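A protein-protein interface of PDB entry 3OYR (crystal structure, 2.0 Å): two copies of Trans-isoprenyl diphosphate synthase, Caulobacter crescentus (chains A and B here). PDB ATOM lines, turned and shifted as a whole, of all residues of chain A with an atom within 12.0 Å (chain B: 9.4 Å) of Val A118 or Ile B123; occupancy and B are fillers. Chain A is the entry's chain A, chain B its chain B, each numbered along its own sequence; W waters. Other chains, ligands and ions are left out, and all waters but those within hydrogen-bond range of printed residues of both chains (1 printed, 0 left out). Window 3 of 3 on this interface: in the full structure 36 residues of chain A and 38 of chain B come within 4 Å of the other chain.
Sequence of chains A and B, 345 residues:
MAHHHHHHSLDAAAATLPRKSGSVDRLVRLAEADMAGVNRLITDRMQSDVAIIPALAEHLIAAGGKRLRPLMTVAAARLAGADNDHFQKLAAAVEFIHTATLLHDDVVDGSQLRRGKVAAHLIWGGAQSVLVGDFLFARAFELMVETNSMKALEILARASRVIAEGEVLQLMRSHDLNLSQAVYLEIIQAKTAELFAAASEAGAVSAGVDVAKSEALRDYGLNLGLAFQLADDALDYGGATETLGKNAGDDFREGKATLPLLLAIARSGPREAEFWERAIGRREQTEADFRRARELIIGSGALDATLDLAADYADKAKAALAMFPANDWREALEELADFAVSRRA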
ATOM      1  N   VAL A 107      25.789 -23.570 -12.156  1.00  0.00           N
ATOM      2  CA  VAL A 107      24.789 -24.417 -12.830  1.00  0.00           C
ATOM      3  C   VAL A 107      23.982 -23.753 -13.971  1.00  0.00           C
ATOM      4  O   VAL A 107      23.632 -24.427 -14.953  1.00  0.00           O
ATOM      5  CB  VAL A 107      23.917 -25.166 -11.750  1.00  0.00           C
ATOM      6  CG1 VAL A 107      22.418 -25.188 -12.065  1.00  0.00           C
ATOM      7  CG2 VAL A 107      24.470 -26.546 -11.502  1.00  0.00           C
ATOM      8  N   VAL A 108      23.717 -22.449 -13.826  1.00  0.00           N
ATOM      9  CA  VAL A 108      23.093 -21.573 -14.851  1.00  0.00           C
ATOM     10  C   VAL A 108      21.860 -22.154 -15.568  1.00  0.00           C
ATOM     11  O   VAL A 108      20.858 -22.501 -14.936  1.00  0.00           O
ATOM     12  CB  VAL A 108      24.150 -21.022 -15.877  1.00  0.00           C
ATOM     13  CG1 VAL A 108      23.484 -20.214 -16.992  1.00  0.00           C
ATOM     14  CG2 VAL A 108      25.203 -20.172 -15.161  1.00  0.00           C
ATOM     15  N   VAL A 118      14.682 -16.351 -16.142  1.00  0.00           N
ATOM     16  CA  VAL A 118      14.530 -17.792 -15.968  1.00  0.00           C
ATOM     17  C   VAL A 118      15.499 -18.542 -16.893  1.00  0.00           C
ATOM     18  O   VAL A 118      15.264 -18.657 -18.101  1.00  0.00           O
ATOM     19  CB  VAL A 118      13.053 -18.240 -16.201  1.00  0.00           C
ATOM     20  CG1 VAL A 118      12.894 -19.757 -16.062  1.00  0.00           C
ATOM     21  CG2 VAL A 118      12.118 -17.518 -15.235  1.00  0.00           C
ATOM     22  N   ALA A 119      16.604 -19.015 -16.319  1.00  0.00           N
ATOM     23  CA  ALA A 119      17.521 -19.912 -17.022  1.00  0.00           C
ATOM     24  C   ALA A 119      17.092 -21.356 -16.744  1.00  0.00           C
ATOM     25  O   ALA A 119      17.458 -21.939 -15.718  1.00  0.00           O
ATOM     26  CB  ALA A 119      18.973 -19.662 -16.591  1.00  0.00           C
ATOM     27  N   ALA A 120      16.303 -21.912 -17.664  1.00  0.00           N
ATOM     28  CA  ALA A 120      15.627 -23.202 -17.466  1.00  0.00           C
ATOM     29  C   ALA A 120      16.559 -24.414 -17.516  1.00  0.00           C
ATOM     30  O   ALA A 120      16.699 -25.133 -16.521  1.00  0.00           O
ATOM     31  CB  ALA A 120      14.474 -23.361 -18.463  1.00  0.00           C
ATOM     32  N   HIS A 121      17.191 -24.636 -18.670  1.00  0.00           N
ATOM     33  CA  HIS A 121      18.077 -25.791 -18.859  1.00  0.00           C
ATOM     34  C   HIS A 121      19.496 -25.584 -18.300  1.00  0.00           C
ATOM     35  O   HIS A 121      19.944 -24.451 -18.080  1.00  0.00           O
ATOM     36  CB  HIS A 121      18.073 -26.309 -20.321  1.00  0.00           C
ATOM     37  CG  HIS A 121      18.328 -25.258 -21.363  1.00  0.00           C
ATOM     38  ND1 HIS A 121      19.491 -25.211 -22.102  1.00  0.00           N
ATOM     39  CD2 HIS A 121      17.554 -24.242 -21.818  1.00  0.00           C
ATOM     40  CE1 HIS A 121      19.433 -24.200 -22.951  1.00  0.00           C
ATOM     41  NE2 HIS A 121      18.268 -23.596 -22.798  1.00  0.00           N
ATOM     42  N   LEU A 122      20.176 -26.699 -18.038  1.00  0.00           N
ATOM     43  CA  LEU A 122      21.532 -26.685 -17.495  1.00  0.00           C
ATOM     44  C   LEU A 122      22.534 -26.427 -18.586  1.00  0.00           C
ATOM     45  O   LEU A 122      22.367 -26.911 -19.711  1.00  0.00           O
ATOM     46  CB  LEU A 122      21.872 -28.041 -16.886  1.00  0.00           C
ATOM     47  CG  LEU A 122      21.100 -28.470 -15.652  1.00  0.00           C
ATOM     48  CD1 LEU A 122      21.008 -29.974 -15.616  1.00  0.00           C
ATOM     49  CD2 LEU A 122      21.767 -27.927 -14.411  1.00  0.00           C
ATOM     50  N   ILE A 123      23.592 -25.694 -18.245  1.00  0.00           N
ATOM     51  CA  ILE A 123      24.758 -25.579 -19.126  1.00  0.00           C
ATOM     52  C   ILE A 123      25.435 -26.953 -19.254  1.00  0.00           C
ATOM     53  O   ILE A 123      25.132 -27.872 -18.481  1.00  0.00           O
ATOM     54  CB  ILE A 123      25.757 -24.468 -18.662  1.00  0.00           C
ATOM     55  CG1 ILE A 123      26.117 -24.600 -17.171  1.00  0.00           C
ATOM     56  CG2 ILE A 123      25.192 -23.078 -18.958  1.00  0.00           C
ATOM     57  CD1 ILE A 123      27.523 -25.109 -16.888  1.00  0.00           C
ATOM     58  N   VAL A 168      19.885 -18.771  -2.103  1.00  0.00           N
ATOM     59  CA  VAL A 168      18.599 -18.423  -2.711  1.00  0.00           C
ATOM     60  C   VAL A 168      18.369 -16.897  -2.647  1.00  0.00           C
ATOM     61  O   VAL A 168      17.986 -16.284  -3.652  1.00  0.00           O
ATOM     62  CB  VAL A 168      17.419 -19.225  -2.083  1.00  0.00           C
ATOM     63  CG1 VAL A 168      16.094 -18.779  -2.647  1.00  0.00           C
ATOM     64  CG2 VAL A 168      17.571 -20.713  -2.359  1.00  0.00           C
ATOM     65  N   LEU A 171      20.452 -14.888  -5.127  1.00  0.00           N
ATOM     66  CA  LEU A 171      19.992 -15.013  -6.493  1.00  0.00           C
ATOM     67  C   LEU A 171      18.718 -14.217  -6.770  1.00  0.00           C
ATOM     68  O   LEU A 171      18.575 -13.655  -7.862  1.00  0.00           O
ATOM     69  CB  LEU A 171      19.840 -16.479  -6.874  1.00  0.00           C
ATOM     70  CG  LEU A 171      20.263 -16.748  -8.316  1.00  0.00           C
ATOM     71  CD1 LEU A 171      21.762 -16.442  -8.532  1.00  0.00           C
ATOM     72  CD2 LEU A 171      19.928 -18.177  -8.677  1.00  0.00           C
ATOM     73  N   MET A 172      17.813 -14.127  -5.787  1.00  0.00           N
ATOM     74  CA  MET A 172      16.660 -13.220  -5.920  1.00  0.00           C
ATOM     75  C   MET A 172      17.024 -11.738  -5.717  1.00  0.00           C
ATOM     76  O   MET A 172      16.179 -10.866  -5.911  1.00  0.00           O
ATOM     77  CB  MET A 172      15.443 -13.642  -5.066  1.00  0.00           C
ATOM     78  CG  MET A 172      15.616 -13.679  -3.544  1.00  0.00           C
ATOM     79  SD  MET A 172      14.155 -14.321  -2.643  1.00  0.00           S
ATOM     80  CE  MET A 172      13.207 -12.832  -2.342  1.00  0.00           C
ATOM     81  N   SER A 174      20.246 -10.756  -7.094  1.00  0.00           N
ATOM     82  CA  SER A 174      21.401 -10.706  -7.992  1.00  0.00           C
ATOM     83  C   SER A 174      21.318  -9.483  -8.903  1.00  0.00           C
ATOM     84  O   SER A 174      22.331  -8.860  -9.227  1.00  0.00           O
ATOM     85  CB  SER A 174      21.469 -11.990  -8.824  1.00  0.00           C
ATOM     86  OG  SER A 174      22.792 -12.497  -8.877  1.00  0.00           O
ATOM     87  N   HIS A 175      20.086  -9.152  -9.284  1.00  0.00           N
ATOM     88  CA  HIS A 175      19.770  -8.013 -10.138  1.00  0.00           C
ATOM     89  C   HIS A 175      19.850  -6.670  -9.401  1.00  0.00           C
ATOM     90  O   HIS A 175      20.049  -5.629 -10.031  1.00  0.00           O
ATOM     91  CB  HIS A 175      18.342  -8.179 -10.688  1.00  0.00           C
ATOM     92  CG  HIS A 175      17.266  -7.867  -9.685  1.00  0.00           C
ATOM     93  ND1 HIS A 175      16.597  -6.660  -9.657  1.00  0.00           N
ATOM     94  CD2 HIS A 175      16.769  -8.592  -8.654  1.00  0.00           C
ATOM     95  CE1 HIS A 175      15.726  -6.662  -8.664  1.00  0.00           C
ATOM     96  NE2 HIS A 175      15.809  -7.823  -8.040  1.00  0.00           N
ATOM     97  N   ILE B  52      11.137 -17.019  -1.923  1.00  0.00           N
ATOM     98  CA  ILE B  52      11.177 -17.967  -3.051  1.00  0.00           C
ATOM     99  C   ILE B  52      11.130 -19.428  -2.557  1.00  0.00           C
ATOM    100  O   ILE B  52      10.445 -20.274  -3.148  1.00  0.00           O
ATOM    101  CB  ILE B  52      12.421 -17.714  -3.963  1.00  0.00           C
ATOM    102  CG1 ILE B  52      12.133 -16.578  -4.961  1.00  0.00           C
ATOM    103  CG2 ILE B  52      12.846 -18.986  -4.724  1.00  0.00           C
ATOM    104  CD1 ILE B  52      13.184 -16.423  -6.077  1.00  0.00           C
ATOM    105  N   ALA B  55       7.624 -20.616  -1.600  1.00  0.00           N
ATOM    106  CA  ALA B  55       6.854 -20.516  -2.853  1.00  0.00           C
ATOM    107  C   ALA B  55       7.182 -21.680  -3.802  1.00  0.00           C
ATOM    108  O   ALA B  55       6.280 -22.385  -4.226  1.00  0.00           O
ATOM    109  CB  ALA B  55       7.084 -19.170  -3.541  1.00  0.00           C
ATOM    110  N   LEU B  56       8.469 -21.903  -4.093  1.00  0.00           N
ATOM    111  CA  LEU B  56       8.884 -23.018  -4.962  1.00  0.00           C
ATOM    112  C   LEU B  56       8.533 -24.383  -4.363  1.00  0.00           C
ATOM    113  O   LEU B  56       8.030 -25.276  -5.067  1.00  0.00           O
ATOM    114  CB  LEU B  56      10.378 -22.921  -5.307  1.00  0.00           C
ATOM    115  CG  LEU B  56      10.949 -23.689  -6.512  1.00  0.00           C
ATOM    116  CD1 LEU B  56      12.281 -23.113  -6.953  1.00  0.00           C
ATOM    117  CD2 LEU B  56      11.151 -25.174  -6.213  1.00  0.00           C
ATOM    118  N   HIS B  59       4.745 -25.134  -4.325  1.00  0.00           N
ATOM    119  CA  HIS B  59       4.296 -25.392  -5.690  1.00  0.00           C
ATOM    120  C   HIS B  59       4.383 -26.905  -5.971  1.00  0.00           C
ATOM    121  O   HIS B  59       3.441 -27.485  -6.506  1.00  0.00           O
ATOM    122  CB  HIS B  59       5.114 -24.581  -6.690  1.00  0.00           C
ATOM    123  CG  HIS B  59       4.843 -24.917  -8.129  1.00  0.00           C
ATOM    124  ND1 HIS B  59       3.888 -24.262  -8.880  1.00  0.00           N
ATOM    125  CD2 HIS B  59       5.424 -25.814  -8.963  1.00  0.00           C
ATOM    126  CE1 HIS B  59       3.881 -24.752 -10.107  1.00  0.00           C
ATOM    127  NE2 HIS B  59       4.798 -25.700 -10.183  1.00  0.00           N
ATOM    128  N   VAL B 107      15.223 -31.116 -13.230  1.00  0.00           N
ATOM    129  CA  VAL B 107      16.171 -30.195 -13.855  1.00  0.00           C
ATOM    130  C   VAL B 107      17.161 -30.945 -14.763  1.00  0.00           C
ATOM    131  O   VAL B 107      17.466 -30.505 -15.872  1.00  0.00           O
ATOM    132  CB  VAL B 107      16.927 -29.356 -12.784  1.00  0.00           C
ATOM    133  CG1 VAL B 107      18.138 -28.650 -13.368  1.00  0.00           C
ATOM    134  CG2 VAL B 107      15.998 -28.344 -12.179  1.00  0.00           C
ATOM    135  N   SER B 111      12.444 -32.372 -17.709  1.00  0.00           N
ATOM    136  CA  SER B 111      10.998 -32.670 -17.712  1.00  0.00           C
ATOM    137  C   SER B 111      10.153 -31.411 -17.522  1.00  0.00           C
ATOM    138  O   SER B 111      10.527 -30.528 -16.753  1.00  0.00           O
ATOM    139  CB  SER B 111      10.659 -33.683 -16.621  1.00  0.00           C
ATOM    140  OG  SER B 111      11.275 -34.933 -16.886  1.00  0.00           O
ATOM    141  N   GLN B 112       9.019 -31.332 -18.219  1.00  0.00           N
ATOM    142  CA  GLN B 112       8.213 -30.106 -18.220  1.00  0.00           C
ATOM    143  C   GLN B 112       7.001 -30.157 -17.283  1.00  0.00           C
ATOM    144  O   GLN B 112       6.448 -29.118 -16.924  1.00  0.00           O
ATOM    145  CB  GLN B 112       7.805 -29.733 -19.650  1.00  0.00           C
ATOM    146  CG  GLN B 112       9.010 -29.471 -20.570  1.00  0.00           C
ATOM    147  CD  GLN B 112       8.643 -29.400 -22.046  1.00  0.00           C
ATOM    148  OE1 GLN B 112       9.390 -29.876 -22.902  1.00  0.00           O
ATOM    149  NE2 GLN B 112       7.492 -28.804 -22.352  1.00  0.00           N
ATOM    150  N   LYS B 117       1.407 -30.073 -12.544  1.00  0.00           N
ATOM    151  CA  LYS B 117       1.802 -28.670 -12.679  1.00  0.00           C
ATOM    152  C   LYS B 117       3.077 -28.590 -13.514  1.00  0.00           C
ATOM    153  O   LYS B 117       3.797 -29.585 -13.666  1.00  0.00           O
ATOM    154  CB  LYS B 117       2.042 -28.015 -11.306  1.00  0.00           C
ATOM    155  CG  LYS B 117       0.787 -27.755 -10.454  1.00  0.00           C
ATOM    156  CD  LYS B 117       1.159 -26.906  -9.229  1.00  0.00           C
ATOM    157  CE  LYS B 117       0.082 -26.906  -8.142  1.00  0.00           C
ATOM    158  NZ  LYS B 117       0.633 -26.505  -6.795  1.00  0.00           N
ATOM    159  N   VAL B 118       3.350 -27.407 -14.049  1.00  0.00           N
ATOM    160  CA  VAL B 118       4.612 -27.112 -14.729  1.00  0.00           C
ATOM    161  C   VAL B 118       5.753 -27.361 -13.737  1.00  0.00           C
ATOM    162  O   VAL B 118       5.603 -27.080 -12.544  1.00  0.00           O
ATOM    163  CB  VAL B 118       4.614 -25.640 -15.267  1.00  0.00           C
ATOM    164  CG1 VAL B 118       4.411 -24.624 -14.125  1.00  0.00           C
ATOM    165  CG2 VAL B 118       5.866 -25.324 -16.049  1.00  0.00           C
ATOM    166  N   ALA B 119       6.851 -27.954 -14.212  1.00  0.00           N
ATOM    167  CA  ALA B 119       8.008 -28.213 -13.362  1.00  0.00           C
ATOM    168  C   ALA B 119       8.584 -26.887 -12.852  1.00  0.00           C
ATOM    169  O   ALA B 119       8.787 -25.953 -13.637  1.00  0.00           O
ATOM    170  CB  ALA B 119       9.054 -28.987 -14.123  1.00  0.00           C
ATOM    171  N   ALA B 120       8.837 -26.823 -11.541  1.00  0.00           N
ATOM    172  CA  ALA B 120       9.278 -25.605 -10.840  1.00  0.00           C
ATOM    173  C   ALA B 120      10.386 -24.810 -11.523  1.00  0.00           C
ATOM    174  O   ALA B 120      10.363 -23.572 -11.510  1.00  0.00           O
ATOM    175  CB  ALA B 120       9.692 -25.947  -9.421  1.00  0.00           C
ATOM    176  N   HIS B 121      11.340 -25.513 -12.136  1.00  0.00           N
ATOM    177  CA  HIS B 121      12.469 -24.864 -12.808  1.00  0.00           C
ATOM    178  C   HIS B 121      12.101 -24.075 -14.066  1.00  0.00           C
ATOM    179  O   HIS B 121      12.905 -23.284 -14.554  1.00  0.00           O
ATOM    180  CB  HIS B 121      13.575 -25.866 -13.121  1.00  0.00           C
ATOM    181  CG  HIS B 121      13.188 -26.922 -14.113  1.00  0.00           C
ATOM    182  ND1 HIS B 121      13.426 -26.797 -15.468  1.00  0.00           N
ATOM    183  CD2 HIS B 121      12.605 -28.134 -13.948  1.00  0.00           C
ATOM    184  CE1 HIS B 121      12.996 -27.879 -16.090  1.00  0.00           C
ATOM    185  NE2 HIS B 121      12.493 -28.707 -15.190  1.00  0.00           N
ATOM    186  N   LEU B 122      10.895 -24.290 -14.588  1.00  0.00           N
ATOM    187  CA  LEU B 122      10.407 -23.496 -15.715  1.00  0.00           C
ATOM    188  C   LEU B 122       9.791 -22.165 -15.264  1.00  0.00           C
ATOM    189  O   LEU B 122       9.638 -21.245 -16.069  1.00  0.00           O
ATOM    190  CB  LEU B 122       9.423 -24.307 -16.575  1.00  0.00           C
ATOM    191  CG  LEU B 122      10.014 -25.448 -17.424  1.00  0.00           C
ATOM    192  CD1 LEU B 122       8.913 -26.293 -18.076  1.00  0.00           C
ATOM    193  CD2 LEU B 122      10.982 -24.932 -18.483  1.00  0.00           C
ATOM    194  N   ILE B 123       9.450 -22.074 -13.978  1.00  0.00           N
ATOM    195  CA  ILE B 123       8.894 -20.863 -13.383  1.00  0.00           C
ATOM    196  C   ILE B 123       9.974 -20.041 -12.662  1.00  0.00           C
ATOM    197  O   ILE B 123      10.066 -18.823 -12.839  1.00  0.00           O
ATOM    198  CB  ILE B 123       7.752 -21.210 -12.388  1.00  0.00           C
ATOM    199  CG1 ILE B 123       6.606 -21.942 -13.089  1.00  0.00           C
ATOM    200  CG2 ILE B 123       7.252 -19.971 -11.650  1.00  0.00           C
ATOM    201  CD1 ILE B 123       6.060 -21.227 -14.347  1.00  0.00           C
ATOM    202  N   TRP B 124      10.790 -20.712 -11.853  1.00  0.00           N
ATOM    203  CA  TRP B 124      11.777 -20.029 -11.016  1.00  0.00           C
ATOM    204  C   TRP B 124      13.198 -20.154 -11.546  1.00  0.00           C
ATOM    205  O   TRP B 124      14.101 -19.462 -11.074  1.00  0.00           O
ATOM    206  CB  TRP B 124      11.703 -20.545  -9.584  1.00  0.00           C
ATOM    207  CG  TRP B 124      10.508 -20.078  -8.820  1.00  0.00           C
ATOM    208  CD1 TRP B 124      10.383 -18.896  -8.144  1.00  0.00           C
ATOM    209  CD2 TRP B 124       9.273 -20.785  -8.625  1.00  0.00           C
ATOM    210  NE1 TRP B 124       9.151 -18.818  -7.549  1.00  0.00           N
ATOM    211  CE2 TRP B 124       8.447 -19.963  -7.826  1.00  0.00           C
ATOM    212  CE3 TRP B 124       8.785 -22.030  -9.049  1.00  0.00           C
ATOM    213  CZ2 TRP B 124       7.149 -20.343  -7.441  1.00  0.00           C
ATOM    214  CZ3 TRP B 124       7.487 -22.414  -8.668  1.00  0.00           C
ATOM    215  CH2 TRP B 124       6.688 -21.566  -7.874  1.00  0.00           C
ATOM    216  N   GLY B 125      13.397 -21.030 -12.530  1.00  0.00           N
ATOM    217  CA  GLY B 125      14.731 -21.265 -13.083  1.00  0.00           C
ATOM    218  C   GLY B 125      15.368 -22.520 -12.514  1.00  0.00           C
ATOM    219  O   GLY B 125      14.996 -22.978 -11.425  1.00  0.00           O
ATOM    220  N   GLY B 126      16.336 -23.056 -13.249  1.00  0.00           N
ATOM    221  CA  GLY B 126      17.075 -24.253 -12.859  1.00  0.00           C
ATOM    222  C   GLY B 126      17.860 -24.052 -11.579  1.00  0.00           C
ATOM    223  O   GLY B 126      17.832 -24.908 -10.689  1.00  0.00           O
ATOM    224  N   ALA B 127      18.536 -22.914 -11.469  1.00  0.00           N
ATOM    225  CA  ALA B 127      19.388 -22.637 -10.312  1.00  0.00           C
ATOM    226  C   ALA B 127      18.586 -22.654  -9.017  1.00  0.00           C
ATOM    227  O   ALA B 127      18.970 -23.352  -8.059  1.00  0.00           O
ATOM    228  CB  ALA B 127      20.123 -21.309 -10.483  1.00  0.00           C
ATOM    229  N   GLN B 128      17.460 -21.933  -9.013  1.00  0.00           N
ATOM    230  CA  GLN B 128      16.594 -21.870  -7.840  1.00  0.00           C
ATOM    231  C   GLN B 128      15.983 -23.219  -7.462  1.00  0.00           C
ATOM    232  O   GLN B 128      15.908 -23.536  -6.274  1.00  0.00           O
ATOM    233  CB  GLN B 128      15.512 -20.776  -7.955  1.00  0.00           C
ATOM    234  CG  GLN B 128      16.025 -19.304  -7.917  1.00  0.00           C
ATOM    235  CD  GLN B 128      16.612 -18.844  -6.566  1.00  0.00           C
ATOM    236  OE1 GLN B 128      17.067 -19.649  -5.756  1.00  0.00           O
ATOM    237  NE2 GLN B 128      16.608 -17.528  -6.338  1.00  0.00           N
ATOM    238  N   SER B 129      15.583 -24.008  -8.459  1.00  0.00           N
ATOM    239  CA  SER B 129      15.162 -25.399  -8.241  1.00  0.00           C
ATOM    240  C   SER B 129      16.215 -26.238  -7.535  1.00  0.00           C
ATOM    241  O   SER B 129      15.928 -26.919  -6.534  1.00  0.00           O
ATOM    242  CB  SER B 129      14.808 -26.074  -9.565  1.00  0.00           C
ATOM    243  OG  SER B 129      13.414 -26.080  -9.752  1.00  0.00           O
HETATM  244  O   HOH W   1      18.032 -20.467 -13.375  1.00  0.00           O
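The backbone carbonyl oxygen of Ala A119 is in hydrogen-bond range of the backbone NH of Gly B126 (2.9 Å).
The side-chain amide nitrogen (NE2) of Gln B128 is in hydrogen-bond range of the backbone carbonyl oxygen (O) of Val A168, 3.3 Å away.
N of His B121 is in hydrogen-bond range of OG of Ser B129 (3.2 Å).
O of Ser B111 is in hydrogen-bond range of NE2 of His B121, 3.1 Å away.
His B121 touches Val A118.
O of Leu B122 touches CG1 of Val A118, 3.6 Å away.
Val A118 touches Ile B123.
Val A118 touches Gly B125.
Ala A119 touches Gly B125 (O to CA, 3.9 Å).
Leu B122 touches Ala A120.
Ala A120 touches Gly B126.
Val B107 touches Leu A122.
Ala B127 touches Leu A171.
Met A172 touches Gln B128 (N to NE2, 3.6 Å).
Of the printed residues of chain B, Val A118 touches His B121, Leu B122, Ile B123 and Gly B125.
Of the printed residues of chain B, Leu A122 touches Val B107.
Of the printed residues of chain A, Val B107 touches Leu A122.
No residue of chain A comes within 4 Å of Val B118.
Ala B119 touches none of the printed residues of chain A.
No residue of chain A comes within 4 Å of Ala B120.
His B121 touches two residues of chain A.
Of chain A, only Val A118 (3.6 Å) and Ala A120 (3.8 Å) come within 4 Å of Leu B122.
Ile B123 touches just one residue of chain A: Val A118.
Of the printed residues of chain A, Gly B125 touches Val A118 and Ala A119.
Of the printed residues of chain A, Gln B128 touches Val A168, Leu A171 and Met A172.
Ser B129 touches none of the printed residues of chain A.
The nearest printed residue of chain B that does not touch Leu A171 is Ile B52 (6.0 Å).
Printed residues of chain B that touch a printed residue of chain A: Ile B52, Val B107, His B121, Leu B122, Ile B123, Gly B125, Gly B126, Ala B127 and Gln B128.
Hydrophobic or aromatic side chains of chain B within 4 Å of the printed part of chain A: Ile B52, Val B107, His B121, Leu B122 and Ala B127.
Of the 13 printed residues of chain A, 7 touch a printed residue of chain B.
Among the printed residues, no Asp or Glu carboxylate lies within 4 Å of a Lys or Arg side-chain nitrogen of the other chain.
Val A118 touches His B121, but with the chains exchanged His A121 does not touch Val B118 (11.6 Å).
Val A118 touches Leu B122, but with the chains exchanged Leu A122 does not touch Val B118 (14.5 Å).
Ala A120 touches His B121, but with the chains exchanged His A121 does not touch Ala B120 (9.9 Å).
Ala A120 touches Leu B122, but with the chains exchanged Leu A122 does not touch Ala B120 (11.9 Å).
Positions printed for both chains: 107, 118, 119, 120, 121, 122 and 123.
Of the 16 pairs that touch across the chains among the printed residues, none has its exchanged pair printed and touching as well.
Water W1 lies within hydrogen-bond range of O of Ala A119, N of Gly B126 and N of Ala B127.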
